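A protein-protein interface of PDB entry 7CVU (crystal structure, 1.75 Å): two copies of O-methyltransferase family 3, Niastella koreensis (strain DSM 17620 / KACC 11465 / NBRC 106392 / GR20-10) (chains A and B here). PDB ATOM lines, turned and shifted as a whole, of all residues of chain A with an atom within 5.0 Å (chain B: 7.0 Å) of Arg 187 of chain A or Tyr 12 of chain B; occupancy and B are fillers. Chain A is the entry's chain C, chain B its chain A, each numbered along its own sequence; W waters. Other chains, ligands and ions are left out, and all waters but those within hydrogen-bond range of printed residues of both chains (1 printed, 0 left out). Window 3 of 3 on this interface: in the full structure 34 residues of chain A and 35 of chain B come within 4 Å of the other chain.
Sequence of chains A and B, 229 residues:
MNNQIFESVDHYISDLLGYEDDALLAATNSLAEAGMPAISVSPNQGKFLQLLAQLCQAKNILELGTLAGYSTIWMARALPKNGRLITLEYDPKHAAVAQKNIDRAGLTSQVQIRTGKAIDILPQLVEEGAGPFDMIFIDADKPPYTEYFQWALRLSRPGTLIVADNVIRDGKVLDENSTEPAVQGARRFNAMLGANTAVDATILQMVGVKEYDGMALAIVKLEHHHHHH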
ATOM      1  N   VAL A 173     -16.526 -17.438  -3.660  1.00  0.00           N
ATOM      2  CA  VAL A 173     -16.350 -16.623  -4.905  1.00  0.00           C
ATOM      3  C   VAL A 173     -16.477 -15.119  -4.617  1.00  0.00           C
ATOM      4  O   VAL A 173     -16.025 -14.296  -5.488  1.00  0.00           O
ATOM      5  CB  VAL A 173     -17.293 -17.061  -6.044  1.00  0.00           C
ATOM      6  CG1 VAL A 173     -16.940 -18.428  -6.509  1.00  0.00           C
ATOM      7  CG2 VAL A 173     -18.777 -16.917  -5.692  1.00  0.00           C
ATOM      8  N   LEU A 174     -17.035 -14.722  -3.474  1.00  0.00           N
ATOM      9  CA  LEU A 174     -17.122 -13.299  -3.070  1.00  0.00           C
ATOM     10  C   LEU A 174     -15.739 -12.738  -2.755  1.00  0.00           C
ATOM     11  O   LEU A 174     -15.608 -11.499  -2.762  1.00  0.00           O
ATOM     12  CB  LEU A 174     -18.026 -13.136  -1.854  1.00  0.00           C
ATOM     13  CG  LEU A 174     -19.480 -13.493  -2.089  1.00  0.00           C
ATOM     14  CD1 LEU A 174     -20.276 -13.281  -0.839  1.00  0.00           C
ATOM     15  CD2 LEU A 174     -20.079 -12.678  -3.222  1.00  0.00           C
ATOM     16  N   ASP A 175     -14.768 -13.593  -2.472  1.00  0.00           N
ATOM     17  CA  ASP A 175     -13.407 -13.168  -2.069  1.00  0.00           C
ATOM     18  C   ASP A 175     -12.552 -12.923  -3.321  1.00  0.00           C
ATOM     19  O   ASP A 175     -11.994 -13.879  -3.858  1.00  0.00           O
ATOM     20  CB  ASP A 175     -12.789 -14.197  -1.134  1.00  0.00           C
ATOM     21  CG  ASP A 175     -11.423 -13.784  -0.621  1.00  0.00           C
ATOM     22  OD1 ASP A 175     -10.959 -12.658  -0.964  1.00  0.00           O
ATOM     23  OD2 ASP A 175     -10.856 -14.600   0.105  1.00  0.00           O
ATOM     24  N   GLU A 176     -12.467 -11.662  -3.780  1.00  0.00           N
ATOM     25  CA  GLU A 176     -11.714 -11.293  -5.001  1.00  0.00           C
ATOM     26  C   GLU A 176     -10.212 -11.568  -4.794  1.00  0.00           C
ATOM     27  O   GLU A 176      -9.538 -11.793  -5.795  1.00  0.00           O
ATOM     28  CB  GLU A 176     -12.076  -9.865  -5.445  1.00  0.00           C
ATOM     29  CG  GLU A 176     -11.483  -8.749  -4.609  1.00  0.00           C
ATOM     30  CD  GLU A 176     -11.670  -7.381  -5.254  1.00  0.00           C
ATOM     31  OE1 GLU A 176     -11.099  -6.401  -4.746  1.00  0.00           O
ATOM     32  OE2 GLU A 176     -12.384  -7.299  -6.279  1.00  0.00           O
ATOM     33  N   VAL A 183     -11.446 -21.565  -6.368  1.00  0.00           N
ATOM     34  CA  VAL A 183     -12.261 -20.342  -6.176  1.00  0.00           C
ATOM     35  C   VAL A 183     -11.932 -19.377  -7.304  1.00  0.00           C
ATOM     36  O   VAL A 183     -12.856 -18.764  -7.823  1.00  0.00           O
ATOM     37  CB  VAL A 183     -12.066 -19.711  -4.794  1.00  0.00           C
ATOM     38  CG1 VAL A 183     -12.771 -18.377  -4.662  1.00  0.00           C
ATOM     39  CG2 VAL A 183     -12.542 -20.653  -3.722  1.00  0.00           C
ATOM     40  N   GLN A 184     -10.645 -19.230  -7.648  1.00  0.00           N
ATOM     41  CA  GLN A 184     -10.268 -18.339  -8.779  1.00  0.00           C
ATOM     42  C   GLN A 184     -10.905 -18.906 -10.064  1.00  0.00           C
ATOM     43  O   GLN A 184     -11.397 -18.099 -10.868  1.00  0.00           O
ATOM     44  CB  GLN A 184      -8.756 -18.246  -8.963  1.00  0.00           C
ATOM     45  CG  GLN A 184      -8.013 -17.616  -7.808  1.00  0.00           C
ATOM     46  CD  GLN A 184      -6.514 -17.689  -8.006  1.00  0.00           C
ATOM     47  OE1 GLN A 184      -5.945 -18.744  -8.284  1.00  0.00           O
ATOM     48  NE2 GLN A 184      -5.860 -16.559  -7.826  1.00  0.00           N
ATOM     49  N   GLY A 185     -10.921 -20.227 -10.245  1.00  0.00           N
ATOM     50  CA  GLY A 185     -11.523 -20.924 -11.396  1.00  0.00           C
ATOM     51  C   GLY A 185     -13.004 -20.594 -11.504  1.00  0.00           C
ATOM     52  O   GLY A 185     -13.451 -20.146 -12.599  1.00  0.00           O
ATOM     53  N   ALA A 186     -13.708 -20.642 -10.378  1.00  0.00           N
ATOM     54  CA  ALA A 186     -15.168 -20.353 -10.327  1.00  0.00           C
ATOM     55  C   ALA A 186     -15.395 -18.874 -10.612  1.00  0.00           C
ATOM     56  O   ALA A 186     -16.297 -18.532 -11.431  1.00  0.00           O
ATOM     57  CB  ALA A 186     -15.733 -20.743  -8.977  1.00  0.00           C
ATOM     58  N   ARG A 187     -14.628 -17.975  -9.976  1.00  0.00           N
ATOM     59  CA  ARG A 187     -14.760 -16.527 -10.217  1.00  0.00           C
ATOM     60  C   ARG A 187     -14.553 -16.220 -11.711  1.00  0.00           C
ATOM     61  O   ARG A 187     -15.286 -15.383 -12.259  1.00  0.00           O
ATOM     62  CB  ARG A 187     -13.791 -15.699  -9.363  1.00  0.00           C
ATOM     63  CG  ARG A 187     -14.165 -15.554  -7.893  1.00  0.00           C
ATOM     64  CD  ARG A 187     -13.199 -14.718  -7.053  1.00  0.00           C
ATOM     65  NE  ARG A 187     -12.951 -13.469  -7.750  1.00  0.00           N
ATOM     66  CZ  ARG A 187     -13.712 -12.384  -7.700  1.00  0.00           C
ATOM     67  NH1 ARG A 187     -14.804 -12.296  -6.953  1.00  0.00           N
ATOM     68  NH2 ARG A 187     -13.378 -11.341  -8.424  1.00  0.00           N
ATOM     69  N   ARG A 188     -13.495 -16.749 -12.325  1.00  0.00           N
ATOM     70  CA  ARG A 188     -13.190 -16.431 -13.735  1.00  0.00           C
ATOM     71  C   ARG A 188     -14.353 -16.951 -14.580  1.00  0.00           C
ATOM     72  O   ARG A 188     -14.762 -16.288 -15.547  1.00  0.00           O
ATOM     73  CB  ARG A 188     -11.852 -17.071 -14.126  1.00  0.00           C
ATOM     74  CG  ARG A 188     -10.652 -16.454 -13.422  1.00  0.00           C
ATOM     75  CD  ARG A 188      -9.361 -17.015 -14.007  1.00  0.00           C
ATOM     76  NE  ARG A 188      -9.213 -18.478 -13.961  1.00  0.00           N
ATOM     77  CZ  ARG A 188      -8.500 -19.171 -13.058  1.00  0.00           C
ATOM     78  NH1 ARG A 188      -7.848 -18.552 -12.087  1.00  0.00           N
ATOM     79  NH2 ARG A 188      -8.442 -20.495 -13.146  1.00  0.00           N
ATOM     80  N   PHE A 189     -14.888 -18.126 -14.252  1.00  0.00           N
ATOM     81  CA  PHE A 189     -15.979 -18.714 -15.049  1.00  0.00           C
ATOM     82  C   PHE A 189     -17.216 -17.814 -14.964  1.00  0.00           C
ATOM     83  O   PHE A 189     -17.851 -17.497 -15.978  1.00  0.00           O
ATOM     84  CB  PHE A 189     -16.233 -20.146 -14.554  1.00  0.00           C
ATOM     85  CG  PHE A 189     -17.448 -20.748 -15.198  1.00  0.00           C
ATOM     86  CD1 PHE A 189     -17.376 -21.334 -16.448  1.00  0.00           C
ATOM     87  CD2 PHE A 189     -18.684 -20.671 -14.576  1.00  0.00           C
ATOM     88  CE1 PHE A 189     -18.500 -21.890 -17.032  1.00  0.00           C
ATOM     89  CE2 PHE A 189     -19.813 -21.175 -15.187  1.00  0.00           C
ATOM     90  CZ  PHE A 189     -19.722 -21.779 -16.422  1.00  0.00           C
ATOM     91  N   ASN A 190     -17.553 -17.350 -13.760  1.00  0.00           N
ATOM     92  CA  ASN A 190     -18.760 -16.514 -13.545  1.00  0.00           C
ATOM     93  C   ASN A 190     -18.559 -15.178 -14.284  1.00  0.00           C
ATOM     94  O   ASN A 190     -19.505 -14.658 -14.869  1.00  0.00           O
ATOM     95  CB  ASN A 190     -19.042 -16.355 -12.054  1.00  0.00           C
ATOM     96  CG  ASN A 190     -19.369 -17.677 -11.371  1.00  0.00           C
ATOM     97  OD1 ASN A 190     -19.752 -18.659 -12.034  1.00  0.00           O
ATOM     98  ND2 ASN A 190     -19.174 -17.720 -10.060  1.00  0.00           N
ATOM     99  N   ALA A 191     -17.371 -14.593 -14.189  1.00  0.00           N
ATOM    100  CA  ALA A 191     -17.044 -13.333 -14.879  1.00  0.00           C
ATOM    101  C   ALA A 191     -17.209 -13.543 -16.379  1.00  0.00           C
ATOM    102  O   ALA A 191     -17.730 -12.634 -17.064  1.00  0.00           O
ATOM    103  CB  ALA A 191     -15.659 -12.855 -14.517  1.00  0.00           C
ATOM    104  N   MET A 192     -16.682 -14.646 -16.882  1.00  0.00           N
ATOM    105  CA  MET A 192     -16.785 -15.013 -18.309  1.00  0.00           C
ATOM    106  C   MET A 192     -18.274 -15.015 -18.685  1.00  0.00           C
ATOM    107  O   MET A 192     -18.639 -14.386 -19.704  1.00  0.00           O
ATOM    108  CB  MET A 192     -16.131 -16.377 -18.543  1.00  0.00           C
ATOM    109  CG  MET A 192     -16.223 -16.804 -19.987  1.00  0.00           C
ATOM    110  SD  MET A 192     -17.761 -17.587 -20.422  1.00  0.00           S
ATOM    111  CE  MET A 192     -17.802 -18.975 -19.293  1.00  0.00           C
ATOM    112  N   GLU B   7     -27.959 -13.714   0.407  1.00  0.00           N
ATOM    113  CA  GLU B   7     -28.206 -12.352  -0.113  1.00  0.00           C
ATOM    114  C   GLU B   7     -26.934 -11.824  -0.795  1.00  0.00           C
ATOM    115  O   GLU B   7     -27.062 -11.197  -1.889  1.00  0.00           O
ATOM    116  CB  GLU B   7     -28.654 -11.404   1.004  1.00  0.00           C
ATOM    117  CG  GLU B   7     -29.884 -11.891   1.720  1.00  0.00           C
ATOM    118  CD  GLU B   7     -30.538 -10.826   2.604  1.00  0.00           C
ATOM    119  OE1 GLU B   7     -30.469  -9.636   2.265  1.00  0.00           O
ATOM    120  OE2 GLU B   7     -31.147 -11.202   3.573  1.00  0.00           O
ATOM    121  N   SER B   8     -25.738 -12.043  -0.224  1.00  0.00           N
ATOM    122  CA  SER B   8     -24.480 -11.452  -0.753  1.00  0.00           C
ATOM    123  C   SER B   8     -24.137 -12.139  -2.079  1.00  0.00           C
ATOM    124  O   SER B   8     -23.758 -11.426  -3.068  1.00  0.00           O
ATOM    125  CB  SER B   8     -23.332 -11.550   0.255  1.00  0.00           C
ATOM    126  OG  SER B   8     -23.615 -10.703   1.379  1.00  0.00           O
ATOM    127  N   VAL B   9     -24.314 -13.463  -2.126  1.00  0.00           N
ATOM    128  CA  VAL B   9     -24.060 -14.270  -3.356  1.00  0.00           C
ATOM    129  C   VAL B   9     -25.086 -13.845  -4.401  1.00  0.00           C
ATOM    130  O   VAL B   9     -24.710 -13.760  -5.552  1.00  0.00           O
ATOM    131  CB  VAL B   9     -24.037 -15.794  -3.110  1.00  0.00           C
ATOM    132  CG1 VAL B   9     -23.973 -16.609  -4.394  1.00  0.00           C
ATOM    133  CG2 VAL B   9     -22.851 -16.156  -2.246  1.00  0.00           C
ATOM    134  N   ASP B  10     -26.333 -13.560  -4.012  1.00  0.00           N
ATOM    135  CA  ASP B  10     -27.361 -13.197  -5.034  1.00  0.00           C
ATOM    136  C   ASP B  10     -27.017 -11.846  -5.657  1.00  0.00           C
ATOM    137  O   ASP B  10     -27.123 -11.704  -6.874  1.00  0.00           O
ATOM    138  CB  ASP B  10     -28.765 -13.163  -4.480  1.00  0.00           C
ATOM    139  CG  ASP B  10     -29.739 -13.864  -5.440  1.00  0.00           C
ATOM    140  OD1 ASP B  10     -29.311 -14.844  -6.159  1.00  0.00           O
ATOM    141  OD2 ASP B  10     -30.867 -13.488  -5.453  1.00  0.00           O
ATOM    142  N   HIS B  11     -26.480 -10.916  -4.882  1.00  0.00           N
ATOM    143  CA  HIS B  11     -26.078  -9.600  -5.434  1.00  0.00           C
ATOM    144  C   HIS B  11     -24.918  -9.785  -6.405  1.00  0.00           C
ATOM    145  O   HIS B  11     -24.856  -9.062  -7.419  1.00  0.00           O
ATOM    146  CB  HIS B  11     -25.755  -8.628  -4.287  1.00  0.00           C
ATOM    147  CG  HIS B  11     -26.988  -8.137  -3.593  1.00  0.00           C
ATOM    148  ND1 HIS B  11     -27.911  -7.311  -4.230  1.00  0.00           N
ATOM    149  CD2 HIS B  11     -27.452  -8.325  -2.337  1.00  0.00           C
ATOM    150  CE1 HIS B  11     -28.897  -7.027  -3.395  1.00  0.00           C
ATOM    151  NE2 HIS B  11     -28.650  -7.649  -2.224  1.00  0.00           N
ATOM    152  N   TYR B  12     -23.969 -10.668  -6.053  1.00  0.00           N
ATOM    153  CA  TYR B  12     -22.816 -11.039  -6.880  1.00  0.00           C
ATOM    154  C   TYR B  12     -23.323 -11.584  -8.219  1.00  0.00           C
ATOM    155  O   TYR B  12     -22.844 -11.164  -9.310  1.00  0.00           O
ATOM    156  CB  TYR B  12     -21.919 -12.017  -6.140  1.00  0.00           C
ATOM    157  CG  TYR B  12     -20.906 -12.783  -6.970  1.00  0.00           C
ATOM    158  CD1 TYR B  12     -19.676 -12.231  -7.301  1.00  0.00           C
ATOM    159  CD2 TYR B  12     -21.187 -14.052  -7.442  1.00  0.00           C
ATOM    160  CE1 TYR B  12     -18.744 -12.948  -8.048  1.00  0.00           C
ATOM    161  CE2 TYR B  12     -20.274 -14.789  -8.184  1.00  0.00           C
ATOM    162  CZ  TYR B  12     -19.052 -14.230  -8.497  1.00  0.00           C
ATOM    163  OH  TYR B  12     -18.110 -14.878  -9.216  1.00  0.00           O
ATOM    164  N   ILE B  13     -24.317 -12.457  -8.134  1.00  0.00           N
ATOM    165  CA  ILE B  13     -24.909 -13.095  -9.343  1.00  0.00           C
ATOM    166  C   ILE B  13     -25.640 -12.024 -10.147  1.00  0.00           C
ATOM    167  O   ILE B  13     -25.444 -11.994 -11.390  1.00  0.00           O
ATOM    168  CB  ILE B  13     -25.793 -14.303  -8.974  1.00  0.00           C
ATOM    169  CG1 ILE B  13     -24.965 -15.453  -8.391  1.00  0.00           C
ATOM    170  CG2 ILE B  13     -26.557 -14.752 -10.219  1.00  0.00           C
ATOM    171  CD1 ILE B  13     -25.805 -16.575  -7.816  1.00  0.00           C
ATOM    172  N   SER B  14     -26.434 -11.136  -9.528  1.00  0.00           N
ATOM    173  CA  SER B  14     -27.264 -10.223 -10.354  1.00  0.00           C
ATOM    174  C   SER B  14     -26.366  -9.151 -10.974  1.00  0.00           C
ATOM    175  O   SER B  14     -26.716  -8.619 -12.056  1.00  0.00           O
ATOM    176  CB  SER B  14     -28.408  -9.609  -9.598  1.00  0.00           C
ATOM    177  OG  SER B  14     -27.942  -9.007  -8.403  1.00  0.00           O
ATOM    178  N   ASP B  15     -25.271  -8.825 -10.307  1.00  0.00           N
ATOM    179  CA  ASP B  15     -24.243  -7.894 -10.841  1.00  0.00           C
ATOM    180  C   ASP B  15     -23.668  -8.448 -12.146  1.00  0.00           C
ATOM    181  O   ASP B  15     -23.378  -7.654 -13.069  1.00  0.00           O
ATOM    182  CB  ASP B  15     -23.183  -7.631  -9.775  1.00  0.00           C
ATOM    183  CG  ASP B  15     -23.590  -6.602  -8.734  1.00  0.00           C
ATOM    184  OD1 ASP B  15     -24.601  -5.920  -8.921  1.00  0.00           O
ATOM    185  OD2 ASP B  15     -22.863  -6.507  -7.727  1.00  0.00           O
ATOM    186  N   LEU B  16     -23.584  -9.779 -12.269  1.00  0.00           N
ATOM    187  CA  LEU B  16     -23.033 -10.431 -13.471  1.00  0.00           C
ATOM    188  C   LEU B  16     -24.139 -10.705 -14.493  1.00  0.00           C
ATOM    189  O   LEU B  16     -23.850 -10.561 -15.729  1.00  0.00           O
ATOM    190  CB  LEU B  16     -22.318 -11.735 -13.075  1.00  0.00           C
ATOM    191  CG  LEU B  16     -21.037 -11.568 -12.276  1.00  0.00           C
ATOM    192  CD1 LEU B  16     -20.619 -12.901 -11.708  1.00  0.00           C
ATOM    193  CD2 LEU B  16     -19.917 -10.993 -13.125  1.00  0.00           C
ATOM    194  N   LEU B  17     -25.304 -11.189 -14.067  1.00  0.00           N
ATOM    195  CA  LEU B  17     -26.239 -11.893 -14.979  1.00  0.00           C
ATOM    196  C   LEU B  17     -27.686 -11.460 -14.763  1.00  0.00           C
ATOM    197  O   LEU B  17     -28.567 -12.171 -15.258  1.00  0.00           O
ATOM    198  CB  LEU B  17     -26.091 -13.392 -14.752  1.00  0.00           C
ATOM    199  CG  LEU B  17     -24.798 -14.002 -15.291  1.00  0.00           C
ATOM    200  CD1 LEU B  17     -24.660 -15.456 -14.818  1.00  0.00           C
ATOM    201  CD2 LEU B  17     -24.752 -14.013 -16.802  1.00  0.00           C
ATOM    202  N   GLY B  18     -27.937 -10.453 -13.923  1.00  0.00           N
ATOM    203  CA  GLY B  18     -29.287 -10.099 -13.470  1.00  0.00           C
ATOM    204  C   GLY B  18     -29.639  -8.644 -13.690  1.00  0.00           C
ATOM    205  O   GLY B  18     -30.296  -8.065 -12.824  1.00  0.00           O
ATOM    206  N   ASN B  44     -32.741 -12.391 -10.267  1.00  0.00           N
ATOM    207  CA  ASN B  44     -32.132 -13.699 -10.654  1.00  0.00           C
ATOM    208  C   ASN B  44     -33.275 -14.712 -10.876  1.00  0.00           C
ATOM    209  O   ASN B  44     -33.167 -15.555 -11.790  1.00  0.00           O
ATOM    210  CB  ASN B  44     -31.074 -14.160  -9.644  1.00  0.00           C
ATOM    211  CG  ASN B  44     -29.818 -13.306  -9.645  1.00  0.00           C
ATOM    212  OD1 ASN B  44     -29.464 -12.655 -10.638  1.00  0.00           O
ATOM    213  ND2 ASN B  44     -29.129 -13.301  -8.512  1.00  0.00           N
HETATM  214  O   HOH W   1     -16.372 -13.471 -10.506  1.00  0.00           O
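O of Val 173 of chain A lies within hydrogen-bond range of NH1 of Arg 187 of chain A, 2.8 Å away.
The backbone carbonyl oxygen (O) of Ala 186 of chain A sits close to the side-chain amide nitrogen (ND2) of Asn 190 of chain A (3.3 Å).
No position is printed for both chains.
Water W1 bridges the side-chain hydroxyl (OH) of Tyr 12 of chain B (2.6 Å) and the backbone carbonyl oxygen (O) of Arg 187 of chain A (2.8 Å).
Of the printed residues of chain B, Val 173 of chain A touches Tyr 12.
Of the printed residues of chain B, Leu 174 of chain A touches Ser 8 (3.7 Å) and Tyr 12 (3.5 Å).
Of chain B, only Tyr 12 (3.9 Å) comes within 4 Å of Arg 187 of chain A.
Printed residues of chain B within 4 Å of Asn 190 of chain A: Tyr 12 and Leu 16.
Printed residues of chain A within 4 Å of Ser 8 of chain B: Leu 174 (3.7 Å).
Tyr 12 of chain B touches four residues of chain A.
Of the printed residues of chain A, Leu 16 of chain B touches Asn 190.
The nearest residue of chain B that does not touch Arg 187 of chain A is Leu 16 of chain B (5.9 Å).
The nearest residue of chain A that does not touch Tyr 12 of chain B is Ala 186 of chain A (4.6 Å).
The nearest printed residue of chain B that does not touch Leu 174 of chain A is Val 9 of chain B (4.1 Å).
The side-chain hydroxyl (OH) of Tyr 12 of chain B lies within hydrogen-bond range of the side-chain amide nitrogen (ND2) of Asn 190 of chain A, at 3.1 Å.
Of the 13 printed residues of chain B, 3 touch a printed residue of chain A.
Hydrophobic or aromatic side chains of chain B within 4 Å of the printed part of chain A: Tyr 12 and Leu 16.
Hydrophobic or aromatic side chains of chain A within 4 Å of the printed part of chain B: Val 173 and Leu 174.
Among the printed residues, no Asp or Glu carboxylate lies within 4 Å of a Lys or Arg side-chain nitrogen of the other chain.
Val 173 of chain A touches Tyr 12 of chain B.
Ser 8 of chain B touches Leu 174 of chain A.
Leu 174 of chain A touches Tyr 12 of chain B (CD2 to CB, 3.5 Å).
CA of Arg 187 of chain A touches OH of Tyr 12 of chain B, 3.9 Å away.
CD1 of Leu 16 of chain B touches O of Asn 190 of chain A, 3.8 Å away.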
